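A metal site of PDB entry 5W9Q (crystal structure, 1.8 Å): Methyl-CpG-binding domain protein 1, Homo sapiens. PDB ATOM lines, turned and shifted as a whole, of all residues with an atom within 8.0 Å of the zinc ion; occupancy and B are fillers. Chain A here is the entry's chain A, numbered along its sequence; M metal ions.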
ATOM      1  N   ARG A   8       2.709  -1.391   3.871  1.00  0.00           N
ATOM      2  CA  ARG A   8       1.364  -0.755   3.895  1.00  0.00           C
ATOM      3  C   ARG A   8       0.935  -0.090   5.237  1.00  0.00           C
ATOM      4  O   ARG A   8      -0.225   0.284   5.367  1.00  0.00           O
ATOM      5  CB  ARG A   8       0.278  -1.732   3.468  1.00  0.00           C
ATOM      6  CG  ARG A   8       0.523  -2.382   2.118  1.00  0.00           C
ATOM      7  CD  ARG A   8       0.336  -1.407   0.983  1.00  0.00           C
ATOM      8  NE  ARG A   8       0.637  -2.045  -0.291  1.00  0.00           N
ATOM      9  CZ  ARG A   8       0.490  -1.480  -1.491  1.00  0.00           C
ATOM     10  NH1 ARG A   8       0.017  -0.244  -1.599  1.00  0.00           N
ATOM     11  NH2 ARG A   8       0.789  -2.164  -2.603  1.00  0.00           N
ATOM     12  N   LYS A   9       1.849   0.078   6.212  1.00  0.00           N
ATOM     13  CA  LYS A   9       1.557   0.877   7.423  1.00  0.00           C
ATOM     14  C   LYS A   9       2.563   1.986   7.530  1.00  0.00           C
ATOM     15  O   LYS A   9       3.759   1.748   7.606  1.00  0.00           O
ATOM     16  CB  LYS A   9       1.578   0.044   8.716  1.00  0.00           C
ATOM     17  CG  LYS A   9       0.701  -1.223   8.687  1.00  0.00           C
ATOM     18  CD  LYS A   9       0.140  -1.526  10.088  1.00  0.00           C
ATOM     19  CE  LYS A   9      -0.285  -2.987  10.206  1.00  0.00           C
ATOM     20  N   CYS A  10       2.071   3.225   7.517  1.00  0.00           N
ATOM     21  CA  CYS A  10       2.912   4.393   7.793  1.00  0.00           C
ATOM     22  C   CYS A  10       3.155   4.474   9.294  1.00  0.00           C
ATOM     23  O   CYS A  10       4.183   5.014   9.766  1.00  0.00           O
ATOM     24  CB  CYS A  10       2.242   5.644   7.289  1.00  0.00           C
ATOM     25  SG  CYS A  10       0.972   6.311   8.391  1.00  0.00           S
ATOM     26  N   GLY A  11       2.165   3.984  10.039  1.00  0.00           N
ATOM     27  CA  GLY A  11       2.277   3.763  11.459  1.00  0.00           C
ATOM     28  C   GLY A  11       1.855   4.930  12.310  1.00  0.00           C
ATOM     29  O   GLY A  11       1.836   4.789  13.507  1.00  0.00           O
ATOM     30  N   ALA A  12       1.521   6.074  11.687  1.00  0.00           N
ATOM     31  CA  ALA A  12       1.298   7.344  12.405  1.00  0.00           C
ATOM     32  C   ALA A  12       0.084   8.108  11.853  1.00  0.00           C
ATOM     33  O   ALA A  12       0.027   9.338  11.920  1.00  0.00           O
ATOM     34  CB  ALA A  12       2.547   8.189  12.274  1.00  0.00           C
ATOM     35  N   CYS A  13      -0.873   7.379  11.273  1.00  0.00           N
ATOM     36  CA  CYS A  13      -2.152   7.938  10.854  1.00  0.00           C
ATOM     37  C   CYS A  13      -3.205   7.248  11.708  1.00  0.00           C
ATOM     38  O   CYS A  13      -2.912   6.273  12.419  1.00  0.00           O
ATOM     39  CB  CYS A  13      -2.367   7.733   9.355  1.00  0.00           C
ATOM     40  SG  CYS A  13      -2.755   6.056   8.810  1.00  0.00           S
ATOM     41  N   ALA A  14      -4.439   7.773  11.662  1.00  0.00           N
ATOM     42  CA  ALA A  14      -5.481   7.331  12.603  1.00  0.00           C
ATOM     43  C   ALA A  14      -5.878   5.920  12.254  1.00  0.00           C
ATOM     44  O   ALA A  14      -6.253   5.168  13.138  1.00  0.00           O
ATOM     45  CB  ALA A  14      -6.702   8.258  12.570  1.00  0.00           C
ATOM     46  N   ALA A  15      -5.799   5.568  10.971  1.00  0.00           N
ATOM     47  CA  ALA A  15      -6.007   4.152  10.565  1.00  0.00           C
ATOM     48  C   ALA A  15      -4.947   3.189  11.116  1.00  0.00           C
ATOM     49  O   ALA A  15      -5.306   2.118  11.659  1.00  0.00           O
ATOM     50  CB  ALA A  15      -6.064   4.032   9.055  1.00  0.00           C
ATOM     51  N   CYS A  16      -3.665   3.554  11.012  1.00  0.00           N
ATOM     52  CA  CYS A  16      -2.593   2.653  11.498  1.00  0.00           C
ATOM     53  C   CYS A  16      -2.646   2.618  13.020  1.00  0.00           C
ATOM     54  O   CYS A  16      -2.446   1.589  13.589  1.00  0.00           O
ATOM     55  CB  CYS A  16      -1.203   3.079  11.023  1.00  0.00           C
ATOM     56  SG  CYS A  16      -0.863   2.840   9.265  1.00  0.00           S
ATOM     57  N   LEU A  17      -2.906   3.770  13.690  1.00  0.00           N
ATOM     58  CA  LEU A  17      -3.019   3.772  15.171  1.00  0.00           C
ATOM     59  C   LEU A  17      -4.220   2.932  15.756  1.00  0.00           C
ATOM     60  O   LEU A  17      -4.207   2.552  16.943  1.00  0.00           O
ATOM     61  CB  LEU A  17      -3.066   5.227  15.745  1.00  0.00           C
ATOM     62  N   LYS A  43      -8.074  -5.919   4.912  1.00  0.00           N
ATOM     63  CA  LYS A  43      -8.209  -5.475   6.284  1.00  0.00           C
ATOM     64  C   LYS A  43      -9.323  -4.460   6.448  1.00  0.00           C
ATOM     65  O   LYS A  43      -9.772  -3.873   5.485  1.00  0.00           O
ATOM     66  CB  LYS A  43      -6.903  -5.012   6.875  1.00  0.00           C
ATOM     67  CG  LYS A  43      -6.186  -3.911   6.235  1.00  0.00           C
ATOM     68  CD  LYS A  43      -5.128  -3.371   7.250  1.00  0.00           C
ATOM     69  CE  LYS A  43      -3.980  -2.757   6.559  1.00  0.00           C
ATOM     70  NZ  LYS A  43      -3.070  -2.163   7.567  1.00  0.00           N
ATOM     71  N   ARG A  47      -8.847   0.513   9.225  1.00  0.00           N
ATOM     72  CA  ARG A  47      -7.439   0.262   9.446  1.00  0.00           C
ATOM     73  C   ARG A  47      -6.596   0.351   8.181  1.00  0.00           C
ATOM     74  O   ARG A  47      -5.415   0.035   8.194  1.00  0.00           O
ATOM     75  CB  ARG A  47      -7.279  -1.087  10.139  1.00  0.00           C
ATOM     76  CG  ARG A  47      -8.154  -1.248  11.396  1.00  0.00           C
ATOM     77  CD  ARG A  47      -8.015  -2.629  12.044  1.00  0.00           C
ATOM     78  NE  ARG A  47      -6.874  -2.676  12.918  1.00  0.00           N
ATOM     79  CZ  ARG A  47      -6.493  -3.728  13.658  1.00  0.00           C
ATOM     80  NH1 ARG A  47      -5.436  -3.602  14.490  1.00  0.00           N
ATOM     81  NH2 ARG A  47      -7.154  -4.865  13.630  1.00  0.00           N
ATOM     82  N   GLN A  48      -7.205   0.751   7.048  1.00  0.00           N
ATOM     83  CA  GLN A  48      -6.453   0.966   5.805  1.00  0.00           C
ATOM     84  C   GLN A  48      -5.629   2.263   5.922  1.00  0.00           C
ATOM     85  O   GLN A  48      -6.191   3.377   6.136  1.00  0.00           O
ATOM     86  CB  GLN A  48      -7.397   1.028   4.649  1.00  0.00           C
ATOM     87  CG  GLN A  48      -8.128  -0.298   4.482  1.00  0.00           C
ATOM     88  CD  GLN A  48      -7.230  -1.351   3.737  1.00  0.00           C
ATOM     89  OE1 GLN A  48      -6.120  -0.993   3.286  1.00  0.00           O
ATOM     90  NE2 GLN A  48      -7.698  -2.607   3.640  1.00  0.00           N
ATOM     91  N   CYS A  49      -4.314   2.126   5.794  1.00  0.00           N
ATOM     92  CA  CYS A  49      -3.412   3.282   5.941  1.00  0.00           C
ATOM     93  C   CYS A  49      -3.726   4.438   4.985  1.00  0.00           C
ATOM     94  O   CYS A  49      -3.839   4.243   3.770  1.00  0.00           O
ATOM     95  CB  CYS A  49      -1.991   2.830   5.695  1.00  0.00           C
ATOM     96  SG  CYS A  49      -0.830   4.218   5.932  1.00  0.00           S
ATOM     97  N   LEU A  50      -3.828   5.657   5.551  1.00  0.00           N
ATOM     98  CA  LEU A  50      -4.193   6.838   4.757  1.00  0.00           C
ATOM     99  C   LEU A  50      -3.075   7.326   3.795  1.00  0.00           C
ATOM    100  O   LEU A  50      -3.344   8.173   2.907  1.00  0.00           O
ATOM    101  CB  LEU A  50      -4.613   8.007   5.706  1.00  0.00           C
ATOM    102  CG  LEU A  50      -5.758   7.650   6.688  1.00  0.00           C
ATOM    103  CD1 LEU A  50      -6.009   8.691   7.728  1.00  0.00           C
ATOM    104  CD2 LEU A  50      -7.022   7.323   5.901  1.00  0.00           C
ATOM    105  N   GLN A  51      -1.826   6.870   4.021  1.00  0.00           N
ATOM    106  CA  GLN A  51      -0.678   7.253   3.172  1.00  0.00           C
ATOM    107  C   GLN A  51      -0.302   6.077   2.210  1.00  0.00           C
ATOM    108  O   GLN A  51      -0.014   6.292   1.012  1.00  0.00           O
ATOM    109  CB  GLN A  51       0.513   7.648   4.060  1.00  0.00           C
ATOM    110  CG  GLN A  51       0.350   8.929   4.889  1.00  0.00           C
ATOM    111  N   PHE A  52      -0.341   4.841   2.711  1.00  0.00           N
ATOM    112  CA  PHE A  52       0.235   3.689   1.960  1.00  0.00           C
ATOM    113  C   PHE A  52      -0.784   2.740   1.333  1.00  0.00           C
ATOM    114  O   PHE A  52      -0.404   2.003   0.421  1.00  0.00           O
ATOM    115  CB  PHE A  52       1.229   2.881   2.815  1.00  0.00           C
ATOM    116  CG  PHE A  52       2.428   3.668   3.328  1.00  0.00           C
ATOM    117  CD1 PHE A  52       2.808   4.912   2.790  1.00  0.00           C
ATOM    118  CD2 PHE A  52       3.226   3.126   4.323  1.00  0.00           C
ATOM    119  CE1 PHE A  52       3.891   5.598   3.274  1.00  0.00           C
ATOM    120  CE2 PHE A  52       4.329   3.819   4.799  1.00  0.00           C
ATOM    121  CZ  PHE A  52       4.669   5.056   4.282  1.00  0.00           C
ATOM    122  N   ALA A  53      -2.038   2.752   1.756  1.00  0.00           N
ATOM    123  CA  ALA A  53      -3.015   1.784   1.211  1.00  0.00           C
ATOM    124  C   ALA A  53      -3.412   2.232  -0.148  1.00  0.00           C
ATOM    125  O   ALA A  53      -3.484   3.435  -0.398  1.00  0.00           O
ATOM    126  CB  ALA A  53      -4.234   1.646   2.058  1.00  0.00           C
HETATM  127 ZN    ZN M   1      -0.831   4.919   8.150  1.00  0.00          ZN
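The zinc ion is bound by SG of Cys 10 (2.3 Å), SG of Cys 49 (2.3 Å), SG of Cys 13 (2.3 Å) and SG of Cys 16 (2.4 Å).
The backbone NH of Gly 11 lies close to the side-chain sulfur of Cys 16 (3.3 Å). SG of Cys 10 sits close to N of Ala 12, 3.3 Å away. SG of Cys 49 lies close to N of Phe 52 (3.3 Å). The backbone NH (N) of Gln 51 lies close to the side-chain sulfur (SG) of Cys 49, 3.4 Å away. N of Ala 15 lies close to SG of Cys 13. The side-chain sulfur (SG) of Cys 13 sits close to the backbone NH (N) of Leu 50, 3.5 Å away.
Merely in contact with the zinc ion: Gly 11 (3.7 Å). Within 4 Å of the zinc ion: Cys 10, Gly 11, Cys 13, Cys 16 and Cys 49. The nearest printed residue that does not touch the zinc ion is Leu 50 (4.04 Å).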
